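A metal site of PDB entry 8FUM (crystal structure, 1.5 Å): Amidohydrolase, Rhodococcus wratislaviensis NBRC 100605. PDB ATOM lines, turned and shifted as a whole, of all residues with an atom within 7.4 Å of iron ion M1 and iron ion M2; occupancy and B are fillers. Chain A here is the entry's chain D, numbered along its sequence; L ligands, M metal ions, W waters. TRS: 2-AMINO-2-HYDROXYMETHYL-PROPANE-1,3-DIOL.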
ATOM      1  N   ASP A  25      13.602 -14.502  22.077  1.00  0.00           N
ATOM      2  CA  ASP A  25      13.300 -13.374  22.972  1.00  0.00           C
ATOM      3  C   ASP A  25      13.981 -13.592  24.317  1.00  0.00           C
ATOM      4  O   ASP A  25      13.477 -14.343  25.166  1.00  0.00           O
ATOM      5  CB  ASP A  25      11.789 -13.219  23.123  1.00  0.00           C
ATOM      6  CG  ASP A  25      11.397 -11.916  23.786  1.00  0.00           C
ATOM      7  OD1 ASP A  25      12.184 -10.964  23.649  1.00  0.00           O
ATOM      8  OD2 ASP A  25      10.337 -11.853  24.439  1.00  0.00           O
ATOM      9  N   ILE A  26      15.081 -12.875  24.508  1.00  0.00           N
ATOM     10  CA  ILE A  26      15.858 -12.844  25.746  1.00  0.00           C
ATOM     11  C   ILE A  26      15.982 -11.390  26.162  1.00  0.00           C
ATOM     12  O   ILE A  26      16.211 -10.526  25.313  1.00  0.00           O
ATOM     13  CB  ILE A  26      17.263 -13.425  25.493  1.00  0.00           C
ATOM     14  CG1 ILE A  26      17.152 -14.857  24.988  1.00  0.00           C
ATOM     15  CG2 ILE A  26      18.095 -13.346  26.749  1.00  0.00           C
ATOM     16  CD1 ILE A  26      18.466 -15.405  24.485  1.00  0.00           C
ATOM     17  N   HIS A  27      15.832 -11.114  27.460  1.00  0.00           N
ATOM     18  CA  HIS A  27      15.813  -9.725  27.934  1.00  0.00           C
ATOM     19  C   HIS A  27      16.995  -9.367  28.828  1.00  0.00           C
ATOM     20  O   HIS A  27      16.896  -9.428  30.060  1.00  0.00           O
ATOM     21  CB  HIS A  27      14.480  -9.416  28.625  1.00  0.00           C
ATOM     22  CG  HIS A  27      13.317  -9.536  27.689  1.00  0.00           C
ATOM     23  ND1 HIS A  27      13.254  -8.830  26.512  1.00  0.00           N
ATOM     24  CD2 HIS A  27      12.197 -10.294  27.728  1.00  0.00           C
ATOM     25  CE1 HIS A  27      12.156  -9.154  25.858  1.00  0.00           C
ATOM     26  NE2 HIS A  27      11.484 -10.026  26.583  1.00  0.00           N
ATOM     27  N   ALA A  71       7.603  -8.942  37.884  1.00  0.00           N
ATOM     28  CA  ALA A  71       7.297  -9.923  36.847  1.00  0.00           C
ATOM     29  C   ALA A  71       8.532 -10.702  36.406  1.00  0.00           C
ATOM     30  O   ALA A  71       8.587 -11.212  35.283  1.00  0.00           O
ATOM     31  CB  ALA A  71       6.595  -9.282  35.639  1.00  0.00           C
ATOM     32  N   GLN A 106      16.557  -8.720  23.163  1.00  0.00           N
ATOM     33  CA  GLN A 106      15.576  -7.657  22.956  1.00  0.00           C
ATOM     34  C   GLN A 106      15.652  -6.798  24.221  1.00  0.00           C
ATOM     35  O   GLN A 106      15.038  -7.110  25.245  1.00  0.00           O
ATOM     36  CB  GLN A 106      14.185  -8.246  22.721  1.00  0.00           C
ATOM     37  CG  GLN A 106      14.147  -9.213  21.538  1.00  0.00           C
ATOM     38  CD  GLN A 106      12.752  -9.476  21.002  1.00  0.00           C
ATOM     39  OE1 GLN A 106      11.840  -8.665  21.178  1.00  0.00           O
ATOM     40  NE2 GLN A 106      12.576 -10.617  20.325  1.00  0.00           N
ATOM     41  N   LEU A 108      14.596  -4.166  26.530  1.00  0.00           N
ATOM     42  CA  LEU A 108      13.329  -3.465  26.762  1.00  0.00           C
ATOM     43  C   LEU A 108      13.449  -2.266  27.687  1.00  0.00           C
ATOM     44  O   LEU A 108      12.435  -1.617  27.970  1.00  0.00           O
ATOM     45  CB  LEU A 108      12.327  -4.431  27.412  1.00  0.00           C
ATOM     46  CG  LEU A 108      11.947  -5.702  26.640  1.00  0.00           C
ATOM     47  CD1 LEU A 108      10.957  -6.531  27.461  1.00  0.00           C
ATOM     48  CD2 LEU A 108      11.360  -5.326  25.267  1.00  0.00           C
ATOM     49  N   THR A 114      11.807  -3.651  34.003  1.00  0.00           N
ATOM     50  CA  THR A 114      11.289  -4.759  33.220  1.00  0.00           C
ATOM     51  C   THR A 114      10.876  -4.354  31.803  1.00  0.00           C
ATOM     52  O   THR A 114      11.214  -5.054  30.844  1.00  0.00           O
ATOM     53  CB  THR A 114      10.114  -5.418  33.951  1.00  0.00           C
ATOM     54  OG1 THR A 114      10.568  -5.883  35.233  1.00  0.00           O
ATOM     55  CG2 THR A 114       9.590  -6.623  33.143  1.00  0.00           C
ATOM     56  N   LEU A 115      10.143  -3.241  31.664  1.00  0.00           N
ATOM     57  CA  LEU A 115       9.610  -2.845  30.355  1.00  0.00           C
ATOM     58  C   LEU A 115       9.465  -1.321  30.306  1.00  0.00           C
ATOM     59  O   LEU A 115       8.477  -0.778  30.809  1.00  0.00           O
ATOM     60  CB  LEU A 115       8.259  -3.526  30.126  1.00  0.00           C
ATOM     61  CG  LEU A 115       7.482  -3.178  28.867  1.00  0.00           C
ATOM     62  CD1 LEU A 115       8.243  -3.545  27.619  1.00  0.00           C
ATOM     63  CD2 LEU A 115       6.110  -3.887  28.949  1.00  0.00           C
ATOM     64  N   HIS A 211       8.095  -6.482  19.647  1.00  0.00           N
ATOM     65  CA  HIS A 211       7.884  -7.052  20.967  1.00  0.00           C
ATOM     66  C   HIS A 211       6.761  -6.326  21.696  1.00  0.00           C
ATOM     67  O   HIS A 211       6.608  -5.101  21.593  1.00  0.00           O
ATOM     68  CB  HIS A 211       9.176  -6.989  21.807  1.00  0.00           C
ATOM     69  CG  HIS A 211       9.112  -7.732  23.108  1.00  0.00           C
ATOM     70  ND1 HIS A 211       8.443  -7.240  24.205  1.00  0.00           N
ATOM     71  CD2 HIS A 211       9.625  -8.935  23.484  1.00  0.00           C
ATOM     72  CE1 HIS A 211       8.553  -8.099  25.211  1.00  0.00           C
ATOM     73  NE2 HIS A 211       9.261  -9.137  24.798  1.00  0.00           N
ATOM     74  N   LEU A 212       5.952  -7.102  22.407  1.00  0.00           N
ATOM     75  CA  LEU A 212       4.968  -6.582  23.336  1.00  0.00           C
ATOM     76  C   LEU A 212       5.457  -5.307  24.012  1.00  0.00           C
ATOM     77  O   LEU A 212       6.603  -5.224  24.479  1.00  0.00           O
ATOM     78  CB  LEU A 212       4.705  -7.676  24.373  1.00  0.00           C
ATOM     79  CG  LEU A 212       3.976  -7.508  25.672  1.00  0.00           C
ATOM     80  CD1 LEU A 212       3.664  -8.917  26.214  1.00  0.00           C
ATOM     81  CD2 LEU A 212       4.786  -6.729  26.682  1.00  0.00           C
ATOM     82  N   HIS A 233      -2.642  -8.007  30.854  1.00  0.00           N
ATOM     83  CA  HIS A 233      -1.726  -8.976  30.293  1.00  0.00           C
ATOM     84  C   HIS A 233      -2.385  -9.753  29.142  1.00  0.00           C
ATOM     85  O   HIS A 233      -1.782  -9.893  28.065  1.00  0.00           O
ATOM     86  CB  HIS A 233      -1.186  -9.855  31.423  1.00  0.00           C
ATOM     87  CG  HIS A 233       0.043 -10.627  31.040  1.00  0.00           C
ATOM     88  ND1 HIS A 233       0.802 -11.308  31.974  1.00  0.00           N
ATOM     89  CD2 HIS A 233       0.631 -10.864  29.842  1.00  0.00           C
ATOM     90  CE1 HIS A 233       1.796 -11.928  31.371  1.00  0.00           C
ATOM     91  NE2 HIS A 233       1.718 -11.682  30.081  1.00  0.00           N
ATOM     92  N   VAL A 264       6.330 -10.840  18.529  1.00  0.00           N
ATOM     93  CA  VAL A 264       7.015 -11.441  19.661  1.00  0.00           C
ATOM     94  C   VAL A 264       6.191 -11.181  20.915  1.00  0.00           C
ATOM     95  O   VAL A 264       6.037 -10.039  21.344  1.00  0.00           O
ATOM     96  CB  VAL A 264       8.463 -10.927  19.806  1.00  0.00           C
ATOM     97  CG1 VAL A 264       9.117 -11.552  21.059  1.00  0.00           C
ATOM     98  CG2 VAL A 264       9.292 -11.248  18.571  1.00  0.00           C
ATOM     99  N   GLU A 265       5.716 -12.271  21.521  1.00  0.00           N
ATOM    100  CA  GLU A 265       5.015 -12.241  22.801  1.00  0.00           C
ATOM    101  C   GLU A 265       3.609 -11.689  22.639  1.00  0.00           C
ATOM    102  O   GLU A 265       3.053 -11.094  23.571  1.00  0.00           O
ATOM    103  CB  GLU A 265       5.823 -11.549  23.898  1.00  0.00           C
ATOM    104  CG  GLU A 265       5.539 -12.078  25.285  1.00  0.00           C
ATOM    105  CD  GLU A 265       6.607 -11.733  26.265  1.00  0.00           C
ATOM    106  OE1 GLU A 265       7.761 -11.642  25.824  1.00  0.00           O
ATOM    107  OE2 GLU A 265       6.273 -11.540  27.457  1.00  0.00           O
ATOM    108  N   GLN A 309       6.318 -17.872  23.165  1.00  0.00           N
ATOM    109  CA  GLN A 309       6.099 -17.595  24.574  1.00  0.00           C
ATOM    110  C   GLN A 309       5.126 -16.436  24.750  1.00  0.00           C
ATOM    111  O   GLN A 309       5.161 -15.470  23.986  1.00  0.00           O
ATOM    112  CB  GLN A 309       7.440 -17.269  25.250  1.00  0.00           C
ATOM    113  CG  GLN A 309       7.399 -17.075  26.749  1.00  0.00           C
ATOM    114  CD  GLN A 309       6.916 -15.709  27.166  1.00  0.00           C
ATOM    115  OE1 GLN A 309       6.900 -14.786  26.356  1.00  0.00           O
ATOM    116  NE2 GLN A 309       6.538 -15.562  28.422  1.00  0.00           N
ATOM    117  N   PRO A 310       4.221 -16.491  25.731  1.00  0.00           N
ATOM    118  CA  PRO A 310       3.931 -17.602  26.635  1.00  0.00           C
ATOM    119  C   PRO A 310       3.064 -18.623  25.929  1.00  0.00           C
ATOM    120  O   PRO A 310       2.022 -18.275  25.374  1.00  0.00           O
ATOM    121  CB  PRO A 310       3.187 -16.924  27.788  1.00  0.00           C
ATOM    122  CG  PRO A 310       2.450 -15.784  27.128  1.00  0.00           C
ATOM    123  CD  PRO A 310       3.377 -15.315  26.021  1.00  0.00           C
ATOM    124  N   ALA A 335      10.712 -19.147  21.830  1.00  0.00           N
ATOM    125  CA  ALA A 335      11.349 -18.165  22.692  1.00  0.00           C
ATOM    126  C   ALA A 335      11.149 -18.566  24.146  1.00  0.00           C
ATOM    127  O   ALA A 335      10.129 -19.164  24.500  1.00  0.00           O
ATOM    128  CB  ALA A 335      10.770 -16.759  22.457  1.00  0.00           C
ATOM    129  N   THR A 336      12.099 -18.203  25.006  1.00  0.00           N
ATOM    130  CA  THR A 336      11.930 -18.454  26.434  1.00  0.00           C
ATOM    131  C   THR A 336      11.349 -17.267  27.195  1.00  0.00           C
ATOM    132  O   THR A 336      10.645 -17.478  28.184  1.00  0.00           O
ATOM    133  CB  THR A 336      13.246 -18.786  27.172  1.00  0.00           C
ATOM    134  OG1 THR A 336      14.141 -17.670  27.127  1.00  0.00           O
ATOM    135  CG2 THR A 336      13.936 -20.044  26.643  1.00  0.00           C
ATOM    136  N   ASP A 337      11.667 -16.036  26.783  1.00  0.00           N
ATOM    137  CA  ASP A 337      11.376 -14.805  27.531  1.00  0.00           C
ATOM    138  C   ASP A 337      12.197 -14.680  28.815  1.00  0.00           C
ATOM    139  O   ASP A 337      11.790 -13.978  29.741  1.00  0.00           O
ATOM    140  CB  ASP A 337       9.885 -14.643  27.818  1.00  0.00           C
ATOM    141  CG  ASP A 337       9.483 -13.192  28.002  1.00  0.00           C
ATOM    142  OD1 ASP A 337      10.108 -12.372  27.317  1.00  0.00           O
ATOM    143  OD2 ASP A 337       8.568 -12.890  28.803  1.00  0.00           O
ATOM    144  N   TYR A 338      13.342 -15.339  28.903  1.00  0.00           N
ATOM    145  CA  TYR A 338      14.190 -15.176  30.067  1.00  0.00           C
ATOM    146  C   TYR A 338      14.518 -13.702  30.276  1.00  0.00           C
ATOM    147  O   TYR A 338      14.905 -13.012  29.322  1.00  0.00           O
ATOM    148  CB  TYR A 338      15.498 -15.947  29.852  1.00  0.00           C
ATOM    149  CG  TYR A 338      16.444 -15.863  31.027  1.00  0.00           C
ATOM    150  CD1 TYR A 338      16.351 -16.741  32.095  1.00  0.00           C
ATOM    151  CD2 TYR A 338      17.441 -14.886  31.063  1.00  0.00           C
ATOM    152  CE1 TYR A 338      17.195 -16.647  33.188  1.00  0.00           C
ATOM    153  CE2 TYR A 338      18.312 -14.783  32.163  1.00  0.00           C
ATOM    154  CZ  TYR A 338      18.181 -15.665  33.216  1.00  0.00           C
ATOM    155  OH  TYR A 338      19.025 -15.601  34.304  1.00  0.00           O
ATOM    156  N   PRO A 339      14.432 -13.176  31.505  1.00  0.00           N
ATOM    157  CA  PRO A 339      14.118 -13.853  32.773  1.00  0.00           C
ATOM    158  C   PRO A 339      12.733 -13.566  33.349  1.00  0.00           C
ATOM    159  O   PRO A 339      12.570 -13.578  34.557  1.00  0.00           O
ATOM    160  CB  PRO A 339      15.200 -13.287  33.708  1.00  0.00           C
ATOM    161  CG  PRO A 339      15.457 -11.874  33.164  1.00  0.00           C
ATOM    162  CD  PRO A 339      14.964 -11.822  31.751  1.00  0.00           C
ATOM    163  N   HIS A 340      11.734 -13.365  32.499  1.00  0.00           N
ATOM    164  CA  HIS A 340      10.408 -13.002  32.997  1.00  0.00           C
ATOM    165  C   HIS A 340       9.714 -14.192  33.662  1.00  0.00           C
ATOM    166  O   HIS A 340      10.041 -15.347  33.430  1.00  0.00           O
ATOM    167  CB  HIS A 340       9.562 -12.415  31.878  1.00  0.00           C
ATOM    168  CG  HIS A 340      10.080 -11.102  31.370  1.00  0.00           C
ATOM    169  ND1 HIS A 340       9.429 -10.364  30.407  1.00  0.00           N
ATOM    170  CD2 HIS A 340      11.170 -10.386  31.742  1.00  0.00           C
ATOM    171  CE1 HIS A 340      10.118  -9.249  30.187  1.00  0.00           C
ATOM    172  NE2 HIS A 340      11.178  -9.241  30.983  1.00  0.00           N
ATOM    173  N   PHE A 341       8.717 -13.884  34.486  1.00  0.00           N
ATOM    174  CA  PHE A 341       8.154 -14.920  35.341  1.00  0.00           C
ATOM    175  C   PHE A 341       7.472 -16.017  34.552  1.00  0.00           C
ATOM    176  O   PHE A 341       7.440 -17.176  35.020  1.00  0.00           O
ATOM    177  CB  PHE A 341       7.178 -14.316  36.344  1.00  0.00           C
ATOM    178  CG  PHE A 341       5.798 -14.088  35.795  1.00  0.00           C
ATOM    179  CD1 PHE A 341       5.526 -12.963  35.063  1.00  0.00           C
ATOM    180  CD2 PHE A 341       4.784 -15.000  36.059  1.00  0.00           C
ATOM    181  CE1 PHE A 341       4.254 -12.753  34.537  1.00  0.00           C
ATOM    182  CE2 PHE A 341       3.516 -14.813  35.552  1.00  0.00           C
ATOM    183  CZ  PHE A 341       3.244 -13.677  34.799  1.00  0.00           C
ATOM    184  N   ASP A 342       6.895 -15.692  33.391  1.00  0.00           N
ATOM    185  CA  ASP A 342       6.215 -16.662  32.552  1.00  0.00           C
ATOM    186  C   ASP A 342       7.133 -17.281  31.492  1.00  0.00           C
ATOM    187  O   ASP A 342       6.659 -17.738  30.437  1.00  0.00           O
ATOM    188  CB  ASP A 342       4.909 -16.080  31.969  1.00  0.00           C
ATOM    189  CG  ASP A 342       5.116 -14.822  31.171  1.00  0.00           C
ATOM    190  OD1 ASP A 342       6.212 -14.230  31.186  1.00  0.00           O
ATOM    191  OD2 ASP A 342       4.127 -14.399  30.522  1.00  0.00           O
ATOM    192  N   PHE A 343       8.437 -17.269  31.756  1.00  0.00           N
ATOM    193  CA  PHE A 343       9.436 -18.029  31.006  1.00  0.00           C
ATOM    194  C   PHE A 343       8.913 -19.392  30.600  1.00  0.00           C
ATOM    195  O   PHE A 343       8.296 -20.094  31.401  1.00  0.00           O
ATOM    196  CB  PHE A 343      10.611 -18.205  31.986  1.00  0.00           C
ATOM    197  CG  PHE A 343      11.656 -19.204  31.560  1.00  0.00           C
ATOM    198  CD1 PHE A 343      11.586 -20.529  31.919  1.00  0.00           C
ATOM    199  CD2 PHE A 343      12.763 -18.774  30.842  1.00  0.00           C
ATOM    200  CE1 PHE A 343      12.570 -21.434  31.527  1.00  0.00           C
ATOM    201  CE2 PHE A 343      13.748 -19.657  30.461  1.00  0.00           C
ATOM    202  CZ  PHE A 343      13.641 -20.995  30.812  1.00  0.00           C
HETATM  203  C   TRS L   1       5.684  -9.478  30.682  1.00  0.00           C
HETATM  204  C1  TRS L   1       5.491 -10.945  31.031  1.00  0.00           C
HETATM  205  C2  TRS L   1       6.597  -8.785  31.696  1.00  0.00           C
HETATM  206  C3  TRS L   1       4.328  -8.783  30.613  1.00  0.00           C
HETATM  207  N   TRS L   1       6.342  -9.374  29.352  1.00  0.00           N
HETATM  208  O1  TRS L   1       6.566 -11.712  30.519  1.00  0.00           O
HETATM  209  O2  TRS L   1       6.998  -7.527  31.172  1.00  0.00           O
HETATM  210  O3  TRS L   1       3.667  -8.909  31.850  1.00  0.00           O
HETATM  211 FE    FE M   1       7.819 -10.976  28.940  1.00  0.00          FE
HETATM  212 FE    FE M   2       9.614 -10.780  26.095  1.00  0.00          FE
HETATM  213  O   HOH W   1       8.690  -9.801  27.684  1.00  0.00           O
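Three residues have an atom within 4 Å of iron ion M1: Glu 265, Asp 337 and His 340.
Iron ion M2 is bound by OE1 of Glu 265 (2.1 Å), OD1 of Asp 337 (2.1 Å), NE2 of His 27 (2.1 Å), water W1 (2.1 Å), OD2 of Asp 25 (2.1 Å) and NE2 of His 211 (2.1 Å). Iron ion M2 has six donor atoms within binding distance.
Iron ion M1 is bound by water W1 (1.9 Å), the side-chain carboxylate (OD2) of Asp 337 (2.1 Å), an oxygen (O1) of the ligand (2.1 Å), the side-chain carboxylate (OE2) of Glu 265 (2.2 Å), a nitrogen (N) of the ligand (2.2 Å) and a ring nitrogen (ND1) of His 340 (2.3 Å).
N of His 27 lies within hydrogen-bond range of O of Tyr 338. OD2 of Asp 337 lies close to NE2 of Gln 309. The side-chain carboxylate (OE1) of Glu 265 sits close to the side-chain amide oxygen (OE1) of Gln 309 (3.3 Å). A ring nitrogen (ND1) of His 27 lies within hydrogen-bond range of the backbone carbonyl oxygen of Gln 106 (2.8 Å). NE2 of Gln 106 lies close to OD1 of Asp 25 (3.4 Å).
Within 4 Å of iron ion M2: Asp 25, His 27, His 211, Glu 265 and Asp 337.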
